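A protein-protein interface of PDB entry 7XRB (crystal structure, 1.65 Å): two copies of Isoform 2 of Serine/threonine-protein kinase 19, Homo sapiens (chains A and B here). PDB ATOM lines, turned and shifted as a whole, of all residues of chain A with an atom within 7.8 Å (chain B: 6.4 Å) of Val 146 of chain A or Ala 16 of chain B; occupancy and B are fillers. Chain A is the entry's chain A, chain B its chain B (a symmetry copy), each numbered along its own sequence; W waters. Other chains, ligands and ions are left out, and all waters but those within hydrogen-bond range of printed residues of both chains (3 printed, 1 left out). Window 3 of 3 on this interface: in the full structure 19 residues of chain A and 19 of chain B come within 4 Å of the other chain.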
ATOM      1  N   VAL A 139     -16.361 -14.113   1.415  1.00  0.00           N
ATOM      2  CA  VAL A 139     -15.091 -14.885   1.518  1.00  0.00           C
ATOM      3  C   VAL A 139     -15.321 -16.283   0.921  1.00  0.00           C
ATOM      4  O   VAL A 139     -14.444 -16.747   0.170  1.00  0.00           O
ATOM      5  CB  VAL A 139     -14.560 -14.946   2.963  1.00  0.00           C
ATOM      6  CG1 VAL A 139     -13.370 -15.878   3.065  1.00  0.00           C
ATOM      7  CG2 VAL A 139     -14.202 -13.566   3.494  1.00  0.00           C
ATOM      8  N   LEU A 144     -13.874 -11.916  -1.693  1.00  0.00           N
ATOM      9  CA  LEU A 144     -12.964 -11.254  -0.726  1.00  0.00           C
ATOM     10  C   LEU A 144     -11.977 -12.279  -0.176  1.00  0.00           C
ATOM     11  O   LEU A 144     -12.376 -13.448   0.045  1.00  0.00           O
ATOM     12  CB  LEU A 144     -13.753 -10.659   0.438  1.00  0.00           C
ATOM     13  CG  LEU A 144     -14.639  -9.449   0.153  1.00  0.00           C
ATOM     14  CD1 LEU A 144     -15.287  -8.971   1.447  1.00  0.00           C
ATOM     15  CD2 LEU A 144     -13.871  -8.313  -0.521  1.00  0.00           C
ATOM     16  N   THR A 145     -10.744 -11.841   0.069  1.00  0.00           N
ATOM     17  CA  THR A 145      -9.734 -12.624   0.825  1.00  0.00           C
ATOM     18  C   THR A 145      -9.188 -11.749   1.951  1.00  0.00           C
ATOM     19  O   THR A 145      -9.113 -10.527   1.775  1.00  0.00           O
ATOM     20  CB  THR A 145      -8.629 -13.185  -0.075  1.00  0.00           C
ATOM     21  OG1 THR A 145      -7.820 -12.115  -0.554  1.00  0.00           O
ATOM     22  CG2 THR A 145      -9.184 -13.954  -1.251  1.00  0.00           C
ATOM     23  N   VAL A 146      -8.824 -12.359   3.070  1.00  0.00           N
ATOM     24  CA  VAL A 146      -8.315 -11.588   4.236  1.00  0.00           C
ATOM     25  C   VAL A 146      -7.020 -10.888   3.819  1.00  0.00           C
ATOM     26  O   VAL A 146      -6.150 -11.539   3.193  1.00  0.00           O
ATOM     27  CB  VAL A 146      -8.111 -12.460   5.485  1.00  0.00           C
ATOM     28  CG1 VAL A 146      -7.620 -11.602   6.638  1.00  0.00           C
ATOM     29  CG2 VAL A 146      -9.377 -13.204   5.870  1.00  0.00           C
ATOM     30  N   ARG A 147      -6.920  -9.598   4.129  1.00  0.00           N
ATOM     31  CA  ARG A 147      -5.701  -8.796   3.875  1.00  0.00           C
ATOM     32  C   ARG A 147      -4.952  -8.642   5.193  1.00  0.00           C
ATOM     33  O   ARG A 147      -3.736  -8.918   5.225  1.00  0.00           O
ATOM     34  CB  ARG A 147      -6.070  -7.441   3.268  1.00  0.00           C
ATOM     35  CG  ARG A 147      -4.918  -6.447   3.275  1.00  0.00           C
ATOM     36  CD  ARG A 147      -5.243  -5.271   2.394  1.00  0.00           C
ATOM     37  NE  ARG A 147      -4.258  -4.204   2.432  1.00  0.00           N
ATOM     38  CZ  ARG A 147      -4.323  -3.131   3.227  1.00  0.00           C
ATOM     39  NH1 ARG A 147      -5.316  -2.979   4.090  1.00  0.00           N
ATOM     40  NH2 ARG A 147      -3.382  -2.206   3.160  1.00  0.00           N
ATOM     41  N   ASP A 148      -5.654  -8.205   6.231  1.00  0.00           N
ATOM     42  CA  ASP A 148      -5.100  -8.110   7.609  1.00  0.00           C
ATOM     43  C   ASP A 148      -6.284  -8.187   8.578  1.00  0.00           C
ATOM     44  O   ASP A 148      -7.419  -8.443   8.119  1.00  0.00           O
ATOM     45  CB  ASP A 148      -4.242  -6.853   7.770  1.00  0.00           C
ATOM     46  CG  ASP A 148      -4.959  -5.550   7.461  1.00  0.00           C
ATOM     47  OD1 ASP A 148      -6.184  -5.488   7.648  1.00  0.00           O
ATOM     48  OD2 ASP A 148      -4.280  -4.605   7.038  1.00  0.00           O
ATOM     49  N   ALA A 149      -6.044  -7.949   9.866  1.00  0.00           N
ATOM     50  CA  ALA A 149      -7.072  -8.113  10.913  1.00  0.00           C
ATOM     51  C   ALA A 149      -8.283  -7.213  10.637  1.00  0.00           C
ATOM     52  O   ALA A 149      -9.344  -7.520  11.176  1.00  0.00           O
ATOM     53  CB  ALA A 149      -6.491  -7.842  12.278  1.00  0.00           C
ATOM     54  N   GLY A 150      -8.151  -6.159   9.822  1.00  0.00           N
ATOM     55  CA  GLY A 150      -9.226  -5.161   9.659  1.00  0.00           C
ATOM     56  C   GLY A 150      -9.629  -4.929   8.217  1.00  0.00           C
ATOM     57  O   GLY A 150     -10.379  -3.950   7.981  1.00  0.00           O
ATOM     58  N   SER A 151      -9.215  -5.776   7.272  1.00  0.00           N
ATOM     59  CA  SER A 151      -9.503  -5.516   5.836  1.00  0.00           C
ATOM     60  C   SER A 151      -9.456  -6.779   4.973  1.00  0.00           C
ATOM     61  O   SER A 151      -8.882  -7.803   5.390  1.00  0.00           O
ATOM     62  CB  SER A 151      -8.574  -4.456   5.295  1.00  0.00           C
ATOM     63  OG  SER A 151      -7.247  -4.941   5.207  1.00  0.00           O
ATOM     64  N   TRP A 152     -10.031  -6.663   3.773  1.00  0.00           N
ATOM     65  CA  TRP A 152     -10.130  -7.761   2.786  1.00  0.00           C
ATOM     66  C   TRP A 152      -9.699  -7.232   1.431  1.00  0.00           C
ATOM     67  O   TRP A 152     -10.084  -6.095   1.090  1.00  0.00           O
ATOM     68  CB  TRP A 152     -11.544  -8.343   2.676  1.00  0.00           C
ATOM     69  CG  TRP A 152     -12.057  -8.979   3.924  1.00  0.00           C
ATOM     70  CD1 TRP A 152     -11.946 -10.281   4.320  1.00  0.00           C
ATOM     71  CD2 TRP A 152     -12.765  -8.304   4.965  1.00  0.00           C
ATOM     72  NE1 TRP A 152     -12.524 -10.457   5.549  1.00  0.00           N
ATOM     73  CE2 TRP A 152     -13.041  -9.258   5.966  1.00  0.00           C
ATOM     74  CE3 TRP A 152     -13.176  -6.982   5.137  1.00  0.00           C
ATOM     75  CZ2 TRP A 152     -13.719  -8.921   7.130  1.00  0.00           C
ATOM     76  CZ3 TRP A 152     -13.858  -6.658   6.280  1.00  0.00           C
ATOM     77  CH2 TRP A 152     -14.132  -7.616   7.257  1.00  0.00           C
ATOM     78  N   TRP A 153      -8.971  -8.044   0.683  1.00  0.00           N
ATOM     79  CA  TRP A 153      -8.673  -7.815  -0.749  1.00  0.00           C
ATOM     80  C   TRP A 153      -9.919  -8.115  -1.574  1.00  0.00           C
ATOM     81  O   TRP A 153     -10.569  -9.151  -1.311  1.00  0.00           O
ATOM     82  CB  TRP A 153      -7.559  -8.738  -1.225  1.00  0.00           C
ATOM     83  CG  TRP A 153      -6.249  -8.561  -0.536  1.00  0.00           C
ATOM     84  CD1 TRP A 153      -5.626  -9.472   0.265  1.00  0.00           C
ATOM     85  CD2 TRP A 153      -5.345  -7.457  -0.676  1.00  0.00           C
ATOM     86  NE1 TRP A 153      -4.417  -8.991   0.674  1.00  0.00           N
ATOM     87  CE2 TRP A 153      -4.205  -7.769   0.101  1.00  0.00           C
ATOM     88  CE3 TRP A 153      -5.372  -6.239  -1.362  1.00  0.00           C
ATOM     89  CZ2 TRP A 153      -3.120  -6.902   0.220  1.00  0.00           C
ATOM     90  CZ3 TRP A 153      -4.290  -5.391  -1.254  1.00  0.00           C
ATOM     91  CH2 TRP A 153      -3.180  -5.718  -0.474  1.00  0.00           C
ATOM     92  N   LEU A 154     -10.178  -7.303  -2.598  1.00  0.00           N
ATOM     93  CA  LEU A 154     -11.028  -7.746  -3.721  1.00  0.00           C
ATOM     94  C   LEU A 154     -10.369  -8.989  -4.316  1.00  0.00           C
ATOM     95  O   LEU A 154      -9.156  -8.956  -4.537  1.00  0.00           O
ATOM     96  CB  LEU A 154     -11.123  -6.636  -4.770  1.00  0.00           C
ATOM     97  CG  LEU A 154     -12.017  -6.954  -5.959  1.00  0.00           C
ATOM     98  CD1 LEU A 154     -13.439  -7.201  -5.497  1.00  0.00           C
ATOM     99  CD2 LEU A 154     -11.971  -5.811  -6.946  1.00  0.00           C
ATOM    100  N   ALA A 155     -11.147 -10.034  -4.562  1.00  0.00           N
ATOM    101  CA  ALA A 155     -10.638 -11.282  -5.145  1.00  0.00           C
ATOM    102  C   ALA A 155     -11.543 -11.742  -6.283  1.00  0.00           C
ATOM    103  O   ALA A 155     -12.726 -11.338  -6.347  1.00  0.00           O
ATOM    104  CB  ALA A 155     -10.497 -12.317  -4.055  1.00  0.00           C
ATOM    105  N   GLU B  10     -10.808 -17.390   5.819  1.00  0.00           N
ATOM    106  CA  GLU B  10      -9.725 -18.428   5.857  1.00  0.00           C
ATOM    107  C   GLU B  10      -8.724 -18.203   4.721  1.00  0.00           C
ATOM    108  O   GLU B  10      -7.533 -18.058   4.986  1.00  0.00           O
ATOM    109  CB  GLU B  10     -10.303 -19.845   5.839  1.00  0.00           C
ATOM    110  CG  GLU B  10      -9.240 -20.923   5.896  1.00  0.00           C
ATOM    111  CD  GLU B  10      -9.718 -22.293   6.349  1.00  0.00           C
ATOM    112  OE1 GLU B  10     -10.043 -22.431   7.543  1.00  0.00           O
ATOM    113  OE2 GLU B  10      -9.769 -23.216   5.507  1.00  0.00           O
ATOM    114  N   PRO B  11      -9.112 -18.132   3.423  1.00  0.00           N
ATOM    115  CA  PRO B  11      -8.127 -17.832   2.385  1.00  0.00           C
ATOM    116  C   PRO B  11      -7.412 -16.508   2.698  1.00  0.00           C
ATOM    117  O   PRO B  11      -8.061 -15.554   3.114  1.00  0.00           O
ATOM    118  CB  PRO B  11      -8.936 -17.772   1.086  1.00  0.00           C
ATOM    119  CG  PRO B  11     -10.174 -18.583   1.401  1.00  0.00           C
ATOM    120  CD  PRO B  11     -10.461 -18.330   2.869  1.00  0.00           C
ATOM    121  N   GLY B  12      -6.090 -16.492   2.532  1.00  0.00           N
ATOM    122  CA  GLY B  12      -5.244 -15.319   2.813  1.00  0.00           C
ATOM    123  C   GLY B  12      -4.804 -15.244   4.270  1.00  0.00           C
ATOM    124  O   GLY B  12      -4.094 -14.294   4.593  1.00  0.00           O
ATOM    125  N   SER B  13      -5.207 -16.198   5.121  1.00  0.00           N
ATOM    126  CA  SER B  13      -4.909 -16.221   6.578  1.00  0.00           C
ATOM    127  C   SER B  13      -3.398 -16.141   6.805  1.00  0.00           C
ATOM    128  O   SER B  13      -2.969 -15.286   7.603  1.00  0.00           O
ATOM    129  CB  SER B  13      -5.478 -17.451   7.247  1.00  0.00           C
ATOM    130  OG  SER B  13      -6.895 -17.388   7.285  1.00  0.00           O
ATOM    131  N   ALA B  14      -2.616 -17.018   6.179  1.00  0.00           N
ATOM    132  CA  ALA B  14      -1.145 -17.059   6.389  1.00  0.00           C
ATOM    133  C   ALA B  14      -0.528 -15.743   5.894  1.00  0.00           C
ATOM    134  O   ALA B  14       0.286 -15.144   6.601  1.00  0.00           O
ATOM    135  CB  ALA B  14      -0.538 -18.266   5.717  1.00  0.00           C
ATOM    136  N   ARG B  15      -0.948 -15.267   4.724  1.00  0.00           N
ATOM    137  CA  ARG B  15      -0.396 -14.019   4.147  1.00  0.00           C
ATOM    138  C   ARG B  15      -0.729 -12.843   5.071  1.00  0.00           C
ATOM    139  O   ARG B  15       0.131 -11.991   5.251  1.00  0.00           O
ATOM    140  CB  ARG B  15      -0.927 -13.820   2.726  1.00  0.00           C
ATOM    141  CG  ARG B  15      -0.318 -12.641   1.980  1.00  0.00           C
ATOM    142  CD  ARG B  15       1.197 -12.693   1.952  1.00  0.00           C
ATOM    143  NE  ARG B  15       1.760 -11.482   1.393  1.00  0.00           N
ATOM    144  CZ  ARG B  15       1.879 -10.320   2.027  1.00  0.00           C
ATOM    145  NH1 ARG B  15       1.503 -10.199   3.293  1.00  0.00           N
ATOM    146  NH2 ARG B  15       2.384  -9.280   1.384  1.00  0.00           N
ATOM    147  N   ALA B  16      -1.941 -12.794   5.626  1.00  0.00           N
ATOM    148  CA  ALA B  16      -2.410 -11.730   6.546  1.00  0.00           C
ATOM    149  C   ALA B  16      -1.612 -11.808   7.851  1.00  0.00           C
ATOM    150  O   ALA B  16      -1.202 -10.753   8.367  1.00  0.00           O
ATOM    151  CB  ALA B  16      -3.900 -11.848   6.798  1.00  0.00           C
ATOM    152  N   ALA B  17      -1.388 -13.018   8.358  1.00  0.00           N
ATOM    153  CA  ALA B  17      -0.546 -13.255   9.554  1.00  0.00           C
ATOM    154  C   ALA B  17       0.850 -12.685   9.279  1.00  0.00           C
ATOM    155  O   ALA B  17       1.365 -11.951  10.123  1.00  0.00           O
ATOM    156  CB  ALA B  17      -0.505 -14.730   9.901  1.00  0.00           C
ATOM    157  N   VAL B  18       1.441 -13.013   8.128  1.00  0.00           N
ATOM    158  CA  VAL B  18       2.810 -12.543   7.767  1.00  0.00           C
ATOM    159  C   VAL B  18       2.826 -11.009   7.784  1.00  0.00           C
ATOM    160  O   VAL B  18       3.735 -10.438   8.386  1.00  0.00           O
ATOM    161  CB  VAL B  18       3.291 -13.115   6.422  1.00  0.00           C
ATOM    162  CG1 VAL B  18       4.480 -12.332   5.874  1.00  0.00           C
ATOM    163  CG2 VAL B  18       3.614 -14.601   6.533  1.00  0.00           C
ATOM    164  N   SER B  19       1.850 -10.359   7.141  1.00  0.00           N
ATOM    165  CA  SER B  19       1.783  -8.879   7.067  1.00  0.00           C
ATOM    166  C   SER B  19       1.675  -8.315   8.496  1.00  0.00           C
ATOM    167  O   SER B  19       2.403  -7.359   8.816  1.00  0.00           O
ATOM    168  CB  SER B  19       0.657  -8.435   6.154  1.00  0.00           C
ATOM    169  OG  SER B  19       0.260  -7.101   6.420  1.00  0.00           O
ATOM    170  N   GLU B  20       0.837  -8.912   9.348  1.00  0.00           N
ATOM    171  CA  GLU B  20       0.659  -8.444  10.753  1.00  0.00           C
ATOM    172  C   GLU B  20       1.981  -8.588  11.523  1.00  0.00           C
ATOM    173  O   GLU B  20       2.364  -7.653  12.238  1.00  0.00           O
ATOM    174  CB  GLU B  20      -0.461  -9.220  11.436  1.00  0.00           C
ATOM    175  CG  GLU B  20      -0.653  -8.836  12.888  1.00  0.00           C
ATOM    176  CD  GLU B  20      -1.987  -9.276  13.471  1.00  0.00           C
ATOM    177  OE1 GLU B  20      -2.943  -9.431  12.683  1.00  0.00           O
ATOM    178  OE2 GLU B  20      -2.074  -9.441  14.711  1.00  0.00           O
ATOM    179  N   LEU B  21       2.664  -9.721  11.368  1.00  0.00           N
ATOM    180  CA  LEU B  21       3.916 -10.009  12.120  1.00  0.00           C
ATOM    181  C   LEU B  21       5.047  -9.124  11.606  1.00  0.00           C
ATOM    182  O   LEU B  21       5.881  -8.692  12.387  1.00  0.00           O
ATOM    183  CB  LEU B  21       4.260 -11.499  12.003  1.00  0.00           C
ATOM    184  CG  LEU B  21       3.270 -12.442  12.687  1.00  0.00           C
ATOM    185  CD1 LEU B  21       3.417 -13.861  12.165  1.00  0.00           C
ATOM    186  CD2 LEU B  21       3.424 -12.403  14.201  1.00  0.00           C
ATOM    187  N   LEU B  46      -0.941 -16.913  15.035  1.00  0.00           N
ATOM    188  CA  LEU B  46      -2.063 -16.148  14.425  1.00  0.00           C
ATOM    189  C   LEU B  46      -2.992 -17.072  13.627  1.00  0.00           C
ATOM    190  O   LEU B  46      -4.174 -16.716  13.459  1.00  0.00           O
ATOM    191  CB  LEU B  46      -1.467 -15.040  13.553  1.00  0.00           C
ATOM    192  CG  LEU B  46      -0.792 -13.891  14.305  1.00  0.00           C
ATOM    193  CD1 LEU B  46      -0.369 -12.805  13.333  1.00  0.00           C
ATOM    194  CD2 LEU B  46      -1.686 -13.295  15.384  1.00  0.00           C
ATOM    195  N   LEU B  60       2.198 -19.778  -0.893  1.00  0.00           N
ATOM    196  CA  LEU B  60       2.906 -18.476  -0.950  1.00  0.00           C
ATOM    197  C   LEU B  60       4.344 -18.707  -1.389  1.00  0.00           C
ATOM    198  O   LEU B  60       4.880 -17.864  -2.116  1.00  0.00           O
ATOM    199  CB  LEU B  60       2.869 -17.808   0.424  1.00  0.00           C
ATOM    200  CG  LEU B  60       1.498 -17.330   0.882  1.00  0.00           C
ATOM    201  CD1 LEU B  60       1.546 -16.922   2.338  1.00  0.00           C
ATOM    202  CD2 LEU B  60       0.991 -16.185   0.028  1.00  0.00           C
HETATM  203  O   HOH W   1      -3.868 -12.051   2.565  1.00  0.00           O
HETATM  204  O   HOH W   2     -10.549 -14.826   3.487  1.00  0.00           O
HETATM  205  O   HOH W   3      -3.600  -7.097  10.978  1.00  0.00           O
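The backbone NH of Val 146 of chain A lies within hydrogen-bond range of the backbone carbonyl oxygen of Pro 11 of chain B (3.3 Å).
Val 139 of chain A touches Pro 11 of chain B.
Val 146 of chain A touches Gly 12 of chain B.
CB of Ala 16 of chain B touches CG1 of Val 146 of chain A (3.7 Å).
Arg 147 of chain A touches Ala 16 of chain B.
Ala 149 of chain A touches Glu 20 of chain B (CB to OE1, 3.9 Å).
Of the 13 printed residues of chain A, 4 touch a printed residue of chain B.
Printed residues of chain A that touch a printed residue of chain B: Val 139, Val 146, Arg 147 and Ala 149.
Hydrophobic or aromatic side chains of chain A within 4 Å of the printed part of chain B: Val 139, Val 146 and Ala 149.
Of the 14 printed residues of chain B, 4 touch a printed residue of chain A.
Hydrophobic or aromatic side chains of chain B that line the printed part of chain A: Pro 11 and Ala 16.
Along chain B the printed residues that touch a printed residue of chain A span positions 11 to 20.
Among the printed residues, 6 pairs touch across the chains.
Among the printed residues, no Asp or Glu carboxylate lies within 4 Å of a Lys or Arg side-chain nitrogen of the other chain.
No position is printed for both chains.
Of the 6 pairs that touch across the chains among the printed residues, none has its exchanged pair printed and touching as well.
Printed residues of chain B within 4 Å of Val 146 of chain A: Pro 11, Gly 12 and Ala 16.
Of the printed residues of chain A, Ala 16 of chain B touches Val 146 and Arg 147.
No residue of chain A comes within 4 Å of Ala 17 of chain B.
Of the printed residues of chain A, Pro 11 of chain B touches Val 139 (3.8 Å) and Val 146 (3.3 Å).
Of the printed residues of chain B, Arg 147 of chain A touches Ala 16.
Printed residues of chain A within 4 Å of Glu 20 of chain B: Ala 149.
Printed residues of chain B within 4 Å of Val 139 of chain A: Pro 11 (3.8 Å).
Trp 153 of chain A touches none of the printed residues of chain B.
The nearest printed residue of chain A that does not touch Ala 16 of chain B is Asp 148 of chain A (4.01 Å).
The nearest printed residue of chain A that does not touch Gly 12 of chain B is Thr 145 of chain A (4.9 Å).
NH1 of Arg 147 of chain A is in salt-bridge range of OD2 of Asp 148 of chain A, 3.5 Å away.
The guanidinium group (NH1) of Arg 147 of chain A is in hydrogen-bond range of the side-chain hydroxyl (OG) of Ser 151 of chain A (3.0 Å).
Water W1 lies within hydrogen-bond range of O of Val 146 of chain A (2.4 Å) and O of Gly 12 of chain B (3.0 Å).
Water W2 lies within hydrogen-bond range of O of Pro 11 of chain B (2.6 Å), N of Val 146 of chain A (3.0 Å) and N of Glu 10 of chain B (3.5 Å).
Water W3 bridges the backbone NH of Ala 149 of chain A and the side-chain carboxylate of Glu 20 of chain B.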
